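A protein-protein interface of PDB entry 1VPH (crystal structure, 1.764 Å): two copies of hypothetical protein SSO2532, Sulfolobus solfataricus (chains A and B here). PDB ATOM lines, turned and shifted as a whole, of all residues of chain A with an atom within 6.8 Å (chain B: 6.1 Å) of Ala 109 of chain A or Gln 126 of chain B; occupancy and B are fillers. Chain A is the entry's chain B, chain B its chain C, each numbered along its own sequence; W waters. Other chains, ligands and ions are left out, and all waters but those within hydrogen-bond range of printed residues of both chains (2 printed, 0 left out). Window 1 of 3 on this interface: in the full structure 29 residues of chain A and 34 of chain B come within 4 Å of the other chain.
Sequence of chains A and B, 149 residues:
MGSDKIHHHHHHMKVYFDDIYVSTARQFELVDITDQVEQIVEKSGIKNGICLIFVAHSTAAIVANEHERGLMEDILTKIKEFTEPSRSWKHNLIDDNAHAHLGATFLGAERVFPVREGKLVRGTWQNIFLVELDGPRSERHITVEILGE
Position printed for both chains: 111. Of the 16 pairs that touch across the chains among the printed residues, none has its exchanged pair printed and touching as well.
The backbone carbonyl oxygen (O) of His 57 of chain A is in hydrogen-bond range of the side-chain amide nitrogen (NE2) of Gln 126 of chain B (3.4 Å). The backbone carbonyl oxygen (O) of Val 55 of chain A lies within hydrogen-bond range of the side-chain amide nitrogen (NE2) of Gln 126 of chain B, at 2.9 Å. O of Ser 58 of chain A is in hydrogen-bond range of ND2 of Asn 65 of chain B. The side-chain hydroxyl (OG1) of Thr 105 of chain A lies within hydrogen-bond range of the side-chain amide nitrogen (ND2) of Asn 65 of chain B, 3.1 Å away. The backbone carbonyl oxygen (O) of Thr 105 of chain A sits at hydrogen-bond distance from the guanidinium group (NH2) of Arg 111 of chain B (3.3 Å).
Printed residues of chain A within 4 Å of Gln 126 of chain B: Phe 54, Val 55, Ala 56, His 57 and Ala 109. Printed residues of chain B within 4 Å of His 57 of chain A: Gln 126 (3.4 Å). Of the printed residues of chain A, Phe 113 of chain B touches Leu 52 (3.9 Å) and Phe 54 (3.5 Å). Printed residues of chain A within 4 Å of Val 121 of chain B: Phe 54 (3.5 Å). Printed residues of chain A within 4 Å of Trp 125 of chain B: Ser 58. Of the printed residues of chain B, Phe 54 of chain A touches Phe 113 (3.5 Å), Val 121 (3.5 Å) and Gln 126 (3.5 Å). The nearest residue of chain B that does not touch Ala 109 of chain A is Arg 111 of chain B (5.0 Å). The nearest printed residue of chain A that does not touch Gln 126 of chain B is Ser 58 of chain A (4.7 Å).
The backbone NH of Asn 127 of chain B sits at hydrogen-bond distance from the backbone carbonyl oxygen of Asn 65 of chain B (2.6 Å). The backbone NH of Glu 66 of chain B sits close to the backbone carbonyl oxygen of Trp 125 of chain B, 3.2 Å away. The backbone NH (N) of Val 55 of chain A is in hydrogen-bond range of the backbone carbonyl oxygen (O) of Ala 109 of chain A. The guanidinium group of Arg 122 of chain B lies within hydrogen-bond range of the backbone carbonyl oxygen of Gln 126 of chain B, 3.0 Å away. OE1 of Gln 126 of chain B lies within hydrogen-bond range of N of Gly 123 of chain B.
CD2 of Leu 52 of chain A touches C of Phe 113 of chain B, 3.9 Å away. CZ of Phe 54 of chain A touches CD2 of Phe 113 of chain B, 3.5 Å away. CZ of Phe 54 of chain A touches O of Val 121 of chain B, 3.5 Å away. CZ of Phe 54 of chain A touches OE1 of Gln 126 of chain B, 3.5 Å away. Ala 56 of chain A touches Arg 122 of chain B. Ala 56 of chain A touches Gln 126 of chain B. Ser 58 of chain A touches Trp 125 of chain B. Ala 104 of chain A touches Asn 65 of chain B (CB to ND2, 3.8 Å). Gln 126 of chain B touches Ala 109 of chain A (NE2 to CB, 3.4 Å). Glu 110 of chain A touches Arg 111 of chain B (OE2 to CA, 3.4 Å).
Water W2 lies within hydrogen-bond range of the backbone carbonyl oxygen (O) of Thr 105 of chain A (2.9 Å), the backbone NH (N) of Ala 64 of chain B (3.1 Å) and the guanidinium group (NE) of Arg 111 of chain B (3.1 Å). Water W1 bridges N of Ala 109 of chain A (2.9 Å) and NE of Arg 111 of chain B (3.2 Å).
Printed residues of chain A that touch a printed residue of chain B: Leu 52, Phe 54, Val 55, Ala 56, His 57, Ser 58, Ala 104, Thr 105, Ala 109 and Glu 110. Of the 15 printed residues of chain B, 8 touch a printed residue of chain A. Printed residues of chain B that touch a printed residue of chain A: Asn 65, Arg 111, Phe 113, Val 121, Arg 122, Gly 123, Trp 125 and Gln 126. Among the printed residues, no Asp or Glu carboxylate lies within 4 Å of a Lys or Arg side-chain nitrogen of the other chain.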
ATOM      1  N   LEU A  52       1.197  -8.965   0.384  1.00  0.00           N
ATOM      2  CA  LEU A  52       0.189  -7.907   0.456  1.00  0.00           C
ATOM      3  C   LEU A  52       0.707  -6.808   1.362  1.00  0.00           C
ATOM      4  O   LEU A  52       1.087  -7.052   2.505  1.00  0.00           O
ATOM      5  CB  LEU A  52      -1.115  -8.498   0.992  1.00  0.00           C
ATOM      6  CG  LEU A  52      -2.317  -7.584   1.264  1.00  0.00           C
ATOM      7  CD1 LEU A  52      -2.774  -6.888  -0.041  1.00  0.00           C
ATOM      8  CD2 LEU A  52      -3.429  -8.373   1.943  1.00  0.00           C
ATOM      9  N   ILE A  53       0.664  -5.566   0.896  1.00  0.00           N
ATOM     10  CA  ILE A  53       0.967  -4.408   1.712  1.00  0.00           C
ATOM     11  C   ILE A  53      -0.305  -3.597   1.712  1.00  0.00           C
ATOM     12  O   ILE A  53      -0.737  -3.177   0.648  1.00  0.00           O
ATOM     13  CB  ILE A  53       2.128  -3.570   1.137  1.00  0.00           C
ATOM     14  CG1 ILE A  53       3.355  -4.480   0.932  1.00  0.00           C
ATOM     15  CG2 ILE A  53       2.450  -2.428   2.050  1.00  0.00           C
ATOM     16  CD1 ILE A  53       3.693  -4.686  -0.522  1.00  0.00           C
ATOM     17  N   PHE A  54      -0.885  -3.391   2.882  1.00  0.00           N
ATOM     18  CA  PHE A  54      -2.241  -2.841   3.049  1.00  0.00           C
ATOM     19  C   PHE A  54      -2.266  -1.749   4.114  1.00  0.00           C
ATOM     20  O   PHE A  54      -1.767  -1.952   5.174  1.00  0.00           O
ATOM     21  CB  PHE A  54      -3.168  -3.962   3.446  1.00  0.00           C
ATOM     22  CG  PHE A  54      -4.571  -3.521   3.724  1.00  0.00           C
ATOM     23  CD1 PHE A  54      -5.506  -3.384   2.687  1.00  0.00           C
ATOM     24  CD2 PHE A  54      -4.953  -3.193   5.000  1.00  0.00           C
ATOM     25  CE1 PHE A  54      -6.798  -2.931   2.941  1.00  0.00           C
ATOM     26  CE2 PHE A  54      -6.269  -2.765   5.262  1.00  0.00           C
ATOM     27  CZ  PHE A  54      -7.175  -2.639   4.231  1.00  0.00           C
ATOM     28  N   VAL A  55      -2.845  -0.595   3.803  1.00  0.00           N
ATOM     29  CA  VAL A  55      -3.035   0.470   4.761  1.00  0.00           C
ATOM     30  C   VAL A  55      -4.534   0.565   5.156  1.00  0.00           C
ATOM     31  O   VAL A  55      -5.410   0.746   4.343  1.00  0.00           O
ATOM     32  CB  VAL A  55      -2.327   1.855   4.315  1.00  0.00           C
ATOM     33  CG1 VAL A  55      -2.992   2.494   3.099  1.00  0.00           C
ATOM     34  CG2 VAL A  55      -2.268   2.878   5.486  1.00  0.00           C
ATOM     35  N   ALA A  56      -4.790   0.432   6.461  1.00  0.00           N
ATOM     36  CA  ALA A  56      -6.146   0.388   6.992  1.00  0.00           C
ATOM     37  C   ALA A  56      -6.529   1.823   7.272  1.00  0.00           C
ATOM     38  O   ALA A  56      -6.828   2.157   8.399  1.00  0.00           O
ATOM     39  CB  ALA A  56      -6.147  -0.430   8.289  1.00  0.00           C
ATOM     40  N   HIS A  57      -6.515   2.667   6.248  1.00  0.00           N
ATOM     41  CA  HIS A  57      -6.840   4.091   6.420  1.00  0.00           C
ATOM     42  C   HIS A  57      -7.470   4.573   5.113  1.00  0.00           C
ATOM     43  O   HIS A  57      -7.118   4.096   4.040  1.00  0.00           O
ATOM     44  CB  HIS A  57      -5.579   4.891   6.778  1.00  0.00           C
ATOM     45  CG  HIS A  57      -5.039   4.569   8.136  1.00  0.00           C
ATOM     46  ND1 HIS A  57      -5.609   5.064   9.291  1.00  0.00           N
ATOM     47  CD2 HIS A  57      -4.013   3.781   8.531  1.00  0.00           C
ATOM     48  CE1 HIS A  57      -4.965   4.580  10.341  1.00  0.00           C
ATOM     49  NE2 HIS A  57      -3.975   3.823   9.909  1.00  0.00           N
ATOM     50  N   SER A  58      -8.380   5.538   5.193  1.00  0.00           N
ATOM     51  CA  SER A  58      -9.061   6.007   4.011  1.00  0.00           C
ATOM     52  C   SER A  58      -8.445   7.278   3.471  1.00  0.00           C
ATOM     53  O   SER A  58      -8.874   7.771   2.459  1.00  0.00           O
ATOM     54  CB  SER A  58     -10.558   6.271   4.312  1.00  0.00           C
ATOM     55  OG  SER A  58     -10.733   7.240   5.319  1.00  0.00           O
ATOM     56  N   ALA A  60      -5.002   7.596   3.237  1.00  0.00           N
ATOM     57  CA  ALA A  60      -3.673   7.183   2.860  1.00  0.00           C
ATOM     58  C   ALA A  60      -3.758   6.061   1.786  1.00  0.00           C
ATOM     59  O   ALA A  60      -4.806   5.477   1.550  1.00  0.00           O
ATOM     60  CB  ALA A  60      -2.892   6.719   4.091  1.00  0.00           C
ATOM     61  N   ALA A  61      -2.649   5.806   1.114  1.00  0.00           N
ATOM     62  CA  ALA A  61      -2.594   4.792   0.066  1.00  0.00           C
ATOM     63  C   ALA A  61      -1.229   4.133   0.065  1.00  0.00           C
ATOM     64  O   ALA A  61      -0.337   4.522   0.830  1.00  0.00           O
ATOM     65  CB  ALA A  61      -2.872   5.430  -1.290  1.00  0.00           C
ATOM     66  N   ILE A  62      -1.107   3.091  -0.740  1.00  0.00           N
ATOM     67  CA  ILE A  62       0.140   2.373  -0.962  1.00  0.00           C
ATOM     68  C   ILE A  62       0.375   2.372  -2.479  1.00  0.00           C
ATOM     69  O   ILE A  62      -0.502   1.964  -3.253  1.00  0.00           O
ATOM     70  CB  ILE A  62       0.135   0.905  -0.487  1.00  0.00           C
ATOM     71  CG1 ILE A  62      -0.081   0.762   1.015  1.00  0.00           C
ATOM     72  CG2 ILE A  62       1.491   0.255  -0.821  1.00  0.00           C
ATOM     73  CD1 ILE A  62       1.017   1.267   1.843  1.00  0.00           C
ATOM     74  N   ALA A 104      -6.864   8.625  -2.124  1.00  0.00           N
ATOM     75  CA  ALA A 104      -6.782   7.262  -1.606  1.00  0.00           C
ATOM     76  C   ALA A 104      -7.712   6.323  -2.392  1.00  0.00           C
ATOM     77  O   ALA A 104      -7.363   5.205  -2.712  1.00  0.00           O
ATOM     78  CB  ALA A 104      -7.140   7.227  -0.120  1.00  0.00           C
ATOM     79  N   THR A 105      -8.896   6.802  -2.717  1.00  0.00           N
ATOM     80  CA  THR A 105      -9.888   6.018  -3.446  1.00  0.00           C
ATOM     81  C   THR A 105      -9.323   5.593  -4.812  1.00  0.00           C
ATOM     82  O   THR A 105      -9.406   4.453  -5.216  1.00  0.00           O
ATOM     83  CB  THR A 105     -11.156   6.841  -3.617  1.00  0.00           C
ATOM     84  OG1 THR A 105     -11.752   7.082  -2.314  1.00  0.00           O
ATOM     85  CG2 THR A 105     -12.167   6.112  -4.536  1.00  0.00           C
ATOM     86  N   LEU A 107      -5.928   5.681  -5.761  1.00  0.00           N
ATOM     87  CA  LEU A 107      -4.630   4.999  -5.733  1.00  0.00           C
ATOM     88  C   LEU A 107      -4.737   3.611  -5.185  1.00  0.00           C
ATOM     89  O   LEU A 107      -3.971   2.713  -5.560  1.00  0.00           O
ATOM     90  CB  LEU A 107      -3.649   5.767  -4.912  1.00  0.00           C
ATOM     91  CG  LEU A 107      -3.228   7.110  -5.543  1.00  0.00           C
ATOM     92  CD1 LEU A 107      -2.424   7.893  -4.632  1.00  0.00           C
ATOM     93  CD2 LEU A 107      -2.526   6.856  -6.832  1.00  0.00           C
ATOM     94  N   GLY A 108      -5.597   3.456  -4.201  1.00  0.00           N
ATOM     95  CA  GLY A 108      -5.810   2.148  -3.583  1.00  0.00           C
ATOM     96  C   GLY A 108      -5.022   1.942  -2.294  1.00  0.00           C
ATOM     97  O   GLY A 108      -3.925   2.462  -2.139  1.00  0.00           O
ATOM     98  N   ALA A 109      -5.573   1.156  -1.389  1.00  0.00           N
ATOM     99  CA  ALA A 109      -4.967   0.974  -0.052  1.00  0.00           C
ATOM    100  C   ALA A 109      -3.971  -0.163  -0.020  1.00  0.00           C
ATOM    101  O   ALA A 109      -3.360  -0.389   1.014  1.00  0.00           O
ATOM    102  CB  ALA A 109      -6.044   0.664   0.974  1.00  0.00           C
ATOM    103  N   GLU A 110      -3.870  -0.911  -1.121  1.00  0.00           N
ATOM    104  CA  GLU A 110      -3.046  -2.114  -1.142  1.00  0.00           C
ATOM    105  C   GLU A 110      -2.289  -2.284  -2.445  1.00  0.00           C
ATOM    106  O   GLU A 110      -2.754  -1.838  -3.517  1.00  0.00           O
ATOM    107  CB  GLU A 110      -3.872  -3.376  -0.847  1.00  0.00           C
ATOM    108  CG  GLU A 110      -4.369  -4.124  -2.068  1.00  0.00           C
ATOM    109  CD  GLU A 110      -5.661  -3.572  -2.646  1.00  0.00           C
ATOM    110  OE1 GLU A 110      -6.198  -2.564  -2.117  1.00  0.00           O
ATOM    111  OE2 GLU A 110      -6.125  -4.159  -3.653  1.00  0.00           O
ATOM    112  N   ARG A 111      -1.111  -2.899  -2.322  1.00  0.00           N
ATOM    113  CA  ARG A 111      -0.410  -3.455  -3.484  1.00  0.00           C
ATOM    114  C   ARG A 111      -0.044  -4.870  -3.179  1.00  0.00           C
ATOM    115  O   ARG A 111       0.155  -5.237  -2.017  1.00  0.00           O
ATOM    116  CB  ARG A 111       0.856  -2.677  -3.838  1.00  0.00           C
ATOM    117  CG  ARG A 111       0.626  -1.255  -4.359  1.00  0.00           C
ATOM    118  CD  ARG A 111      -0.060  -1.329  -5.722  1.00  0.00           C
ATOM    119  NE  ARG A 111      -0.229  -0.030  -6.321  1.00  0.00           N
ATOM    120  CZ  ARG A 111      -1.244   0.780  -6.049  1.00  0.00           C
ATOM    121  NH1 ARG A 111      -2.134   0.436  -5.136  1.00  0.00           N
ATOM    122  NH2 ARG A 111      -1.358   1.963  -6.673  1.00  0.00           N
ATOM    123  N   THR B  34     -19.800  -3.481   2.251  1.00  0.00           N
ATOM    124  CA  THR B  34     -18.901  -3.865   3.339  1.00  0.00           C
ATOM    125  C   THR B  34     -19.459  -4.989   4.229  1.00  0.00           C
ATOM    126  O   THR B  34     -18.769  -5.986   4.475  1.00  0.00           O
ATOM    127  CB  THR B  34     -18.505  -2.655   4.280  1.00  0.00           C
ATOM    128  OG1 THR B  34     -18.137  -1.504   3.510  1.00  0.00           O
ATOM    129  CG2 THR B  34     -17.368  -3.077   5.182  1.00  0.00           C
ATOM    130  N   ALA B  64     -12.388   1.342  -1.952  1.00  0.00           N
ATOM    131  CA  ALA B  64     -12.636   1.372  -0.524  1.00  0.00           C
ATOM    132  C   ALA B  64     -12.388   2.771   0.044  1.00  0.00           C
ATOM    133  O   ALA B  64     -11.370   3.439  -0.259  1.00  0.00           O
ATOM    134  CB  ALA B  64     -11.789   0.329   0.162  1.00  0.00           C
ATOM    135  N   ASN B  65     -13.392   3.297   0.720  1.00  0.00           N
ATOM    136  CA  ASN B  65     -13.234   4.592   1.369  1.00  0.00           C
ATOM    137  C   ASN B  65     -14.332   4.808   2.382  1.00  0.00           C
ATOM    138  O   ASN B  65     -15.006   3.858   2.751  1.00  0.00           O
ATOM    139  CB  ASN B  65     -13.098   5.723   0.371  1.00  0.00           C
ATOM    140  CG  ASN B  65     -12.075   6.676   0.812  1.00  0.00           C
ATOM    141  OD1 ASN B  65     -12.406   7.655   1.495  1.00  0.00           O
ATOM    142  ND2 ASN B  65     -10.770   6.337   0.557  1.00  0.00           N
ATOM    143  N   GLU B  66     -14.468   6.041   2.866  1.00  0.00           N
ATOM    144  CA  GLU B  66     -15.354   6.322   3.953  1.00  0.00           C
ATOM    145  C   GLU B  66     -16.780   6.518   3.513  1.00  0.00           C
ATOM    146  O   GLU B  66     -17.050   7.288   2.579  1.00  0.00           O
ATOM    147  CB  GLU B  66     -14.906   7.581   4.700  1.00  0.00           C
ATOM    148  CG  GLU B  66     -15.709   7.791   5.965  1.00  0.00           C
ATOM    149  CD  GLU B  66     -15.213   8.941   6.816  1.00  0.00           C
ATOM    150  OE1 GLU B  66     -14.043   9.392   6.672  1.00  0.00           O
ATOM    151  OE2 GLU B  66     -16.034   9.381   7.656  1.00  0.00           O
ATOM    152  N   HIS B  67     -17.702   5.857   4.226  1.00  0.00           N
ATOM    153  CA  HIS B  67     -19.109   6.004   3.931  1.00  0.00           C
ATOM    154  C   HIS B  67     -19.616   7.280   4.562  1.00  0.00           C
ATOM    155  O   HIS B  67     -20.049   7.255   5.707  1.00  0.00           O
ATOM    156  CB  HIS B  67     -19.919   4.837   4.476  1.00  0.00           C
ATOM    157  CG  HIS B  67     -21.304   4.788   3.941  1.00  0.00           C
ATOM    158  ND1 HIS B  67     -21.795   3.694   3.258  1.00  0.00           N
ATOM    159  CD2 HIS B  67     -22.323   5.690   4.006  1.00  0.00           C
ATOM    160  CE1 HIS B  67     -23.066   3.917   2.947  1.00  0.00           C
ATOM    161  NE2 HIS B  67     -23.400   5.128   3.361  1.00  0.00           N
ATOM    162  N   ARG B 111     -10.221  -5.203  -5.212  1.00  0.00           N
ATOM    163  CA  ARG B 111      -9.456  -4.796  -4.093  1.00  0.00           C
ATOM    164  C   ARG B 111      -9.159  -6.050  -3.267  1.00  0.00           C
ATOM    165  O   ARG B 111      -9.907  -7.006  -3.280  1.00  0.00           O
ATOM    166  CB  ARG B 111     -10.200  -3.742  -3.286  1.00  0.00           C
ATOM    167  CG  ARG B 111     -10.303  -2.367  -3.879  1.00  0.00           C
ATOM    168  CD  ARG B 111      -8.933  -1.722  -4.117  1.00  0.00           C
ATOM    169  NE  ARG B 111      -9.123  -0.369  -4.613  1.00  0.00           N
ATOM    170  CZ  ARG B 111      -9.214  -0.009  -5.881  1.00  0.00           C
ATOM    171  NH1 ARG B 111      -9.124  -0.895  -6.852  1.00  0.00           N
ATOM    172  NH2 ARG B 111      -9.374   1.284  -6.180  1.00  0.00           N
ATOM    173  N   PHE B 113      -8.021  -7.392   0.589  1.00  0.00           N
ATOM    174  CA  PHE B 113      -7.928  -7.044   2.012  1.00  0.00           C
ATOM    175  C   PHE B 113      -7.256  -8.207   2.782  1.00  0.00           C
ATOM    176  O   PHE B 113      -7.389  -9.370   2.388  1.00  0.00           O
ATOM    177  CB  PHE B 113      -9.306  -6.802   2.636  1.00  0.00           C
ATOM    178  CG  PHE B 113      -9.911  -5.471   2.317  1.00  0.00           C
ATOM    179  CD1 PHE B 113     -10.382  -5.214   1.065  1.00  0.00           C
ATOM    180  CD2 PHE B 113     -10.001  -4.487   3.301  1.00  0.00           C
ATOM    181  CE1 PHE B 113     -10.909  -3.988   0.756  1.00  0.00           C
ATOM    182  CE2 PHE B 113     -10.536  -3.260   3.011  1.00  0.00           C
ATOM    183  CZ  PHE B 113     -11.007  -3.012   1.732  1.00  0.00           C
ATOM    184  N   VAL B 121      -9.423  -7.170   7.843  1.00  0.00           N
ATOM    185  CA  VAL B 121      -8.617  -6.075   8.353  1.00  0.00           C
ATOM    186  C   VAL B 121      -8.972  -4.853   7.552  1.00  0.00           C
ATOM    187  O   VAL B 121      -8.831  -4.873   6.333  1.00  0.00           O
ATOM    188  CB  VAL B 121      -7.110  -6.393   8.234  1.00  0.00           C
ATOM    189  CG1 VAL B 121      -6.250  -5.201   8.605  1.00  0.00           C
ATOM    190  CG2 VAL B 121      -6.764  -7.614   9.139  1.00  0.00           C
ATOM    191  N   ARG B 122      -9.466  -3.822   8.224  1.00  0.00           N
ATOM    192  CA  ARG B 122      -9.771  -2.574   7.574  1.00  0.00           C
ATOM    193  C   ARG B 122      -9.931  -1.464   8.567  1.00  0.00           C
ATOM    194  O   ARG B 122     -10.226  -1.686   9.753  1.00  0.00           O
ATOM    195  CB  ARG B 122     -11.031  -2.714   6.771  1.00  0.00           C
ATOM    196  CG  ARG B 122     -12.247  -2.921   7.591  1.00  0.00           C
ATOM    197  CD  ARG B 122     -13.399  -3.202   6.682  1.00  0.00           C
ATOM    198  NE  ARG B 122     -14.562  -3.371   7.495  1.00  0.00           N
ATOM    199  CZ  ARG B 122     -15.304  -2.382   7.966  1.00  0.00           C
ATOM    200  NH1 ARG B 122     -15.049  -1.106   7.677  1.00  0.00           N
ATOM    201  NH2 ARG B 122     -16.329  -2.691   8.746  1.00  0.00           N
ATOM    202  N   GLY B 123      -9.781  -0.246   8.092  1.00  0.00           N
ATOM    203  CA  GLY B 123      -9.894   0.882   8.991  1.00  0.00           C
ATOM    204  C   GLY B 123     -11.329   1.112   9.410  1.00  0.00           C
ATOM    205  O   GLY B 123     -12.286   0.632   8.769  1.00  0.00           O
ATOM    206  N   THR B 124     -11.464   1.891  10.493  1.00  0.00           N
ATOM    207  CA  THR B 124     -12.768   2.328  10.945  1.00  0.00           C
ATOM    208  C   THR B 124     -13.547   2.995   9.799  1.00  0.00           C
ATOM    209  O   THR B 124     -14.761   2.797   9.711  1.00  0.00           O
ATOM    210  CB  THR B 124     -12.646   3.247  12.180  1.00  0.00           C
ATOM    211  OG1 THR B 124     -11.881   2.579  13.207  1.00  0.00           O
ATOM    212  CG2 THR B 124     -14.020   3.653  12.718  1.00  0.00           C
ATOM    213  N   TRP B 125     -12.870   3.771   8.940  1.00  0.00           N
ATOM    214  CA  TRP B 125     -13.565   4.552   7.908  1.00  0.00           C
ATOM    215  C   TRP B 125     -13.239   4.060   6.492  1.00  0.00           C
ATOM    216  O   TRP B 125     -13.303   4.807   5.535  1.00  0.00           O
ATOM    217  CB  TRP B 125     -13.315   6.033   8.137  1.00  0.00           C
ATOM    218  CG  TRP B 125     -13.858   6.413   9.496  1.00  0.00           C
ATOM    219  CD1 TRP B 125     -15.185   6.535   9.862  1.00  0.00           C
ATOM    220  CD2 TRP B 125     -13.100   6.628  10.670  1.00  0.00           C
ATOM    221  NE1 TRP B 125     -15.276   6.855  11.184  1.00  0.00           N
ATOM    222  CE2 TRP B 125     -14.009   6.924  11.705  1.00  0.00           C
ATOM    223  CE3 TRP B 125     -11.735   6.631  10.946  1.00  0.00           C
ATOM    224  CZ2 TRP B 125     -13.592   7.207  12.999  1.00  0.00           C
ATOM    225  CZ3 TRP B 125     -11.322   6.916  12.211  1.00  0.00           C
ATOM    226  CH2 TRP B 125     -12.241   7.198  13.235  1.00  0.00           C
ATOM    227  N   GLN B 126     -12.987   2.752   6.404  1.00  0.00           N
ATOM    228  CA  GLN B 126     -12.651   2.112   5.183  1.00  0.00           C
ATOM    229  C   GLN B 126     -13.732   1.118   4.788  1.00  0.00           C
ATOM    230  O   GLN B 126     -13.698  -0.039   5.177  1.00  0.00           O
ATOM    231  CB  GLN B 126     -11.332   1.376   5.405  1.00  0.00           C
ATOM    232  CG  GLN B 126     -10.610   1.015   4.175  1.00  0.00           C
ATOM    233  CD  GLN B 126      -9.183   0.581   4.490  1.00  0.00           C
ATOM    234  OE1 GLN B 126      -8.931   0.038   5.559  1.00  0.00           O
ATOM    235  NE2 GLN B 126      -8.233   0.879   3.586  1.00  0.00           N
ATOM    236  N   ASN B 127     -14.708   1.574   4.005  1.00  0.00           N
ATOM    237  CA  ASN B 127     -15.822   0.716   3.607  1.00  0.00           C
ATOM    238  C   ASN B 127     -15.581   0.313   2.163  1.00  0.00           C
ATOM    239  O   ASN B 127     -14.859   1.006   1.420  1.00  0.00           O
ATOM    240  CB  ASN B 127     -17.142   1.477   3.766  1.00  0.00           C
ATOM    241  CG  ASN B 127     -17.605   1.546   5.229  1.00  0.00           C
ATOM    242  OD1 ASN B 127     -16.808   1.673   6.173  1.00  0.00           O
ATOM    243  ND2 ASN B 127     -18.889   1.396   5.416  1.00  0.00           N
ATOM    244  N   ILE B 128     -16.218  -0.781   1.761  1.00  0.00           N
ATOM    245  CA  ILE B 128     -16.019  -1.346   0.431  1.00  0.00           C
ATOM    246  C   ILE B 128     -17.204  -0.993  -0.459  1.00  0.00           C
ATOM    247  O   ILE B 128     -18.374  -1.225  -0.079  1.00  0.00           O
ATOM    248  CB  ILE B 128     -15.915  -2.840   0.498  1.00  0.00           C
ATOM    249  CG1 ILE B 128     -14.783  -3.261   1.449  1.00  0.00           C
ATOM    250  CG2 ILE B 128     -15.665  -3.379  -0.886  1.00  0.00           C
ATOM    251  CD1 ILE B 128     -14.581  -4.730   1.576  1.00  0.00           C
HETATM  252  O   HOH W   1      -8.424   0.745  -1.665  1.00  0.00           O
HETATM  253  O   HOH W   2      -9.824   2.336  -3.295  1.00  0.00           O
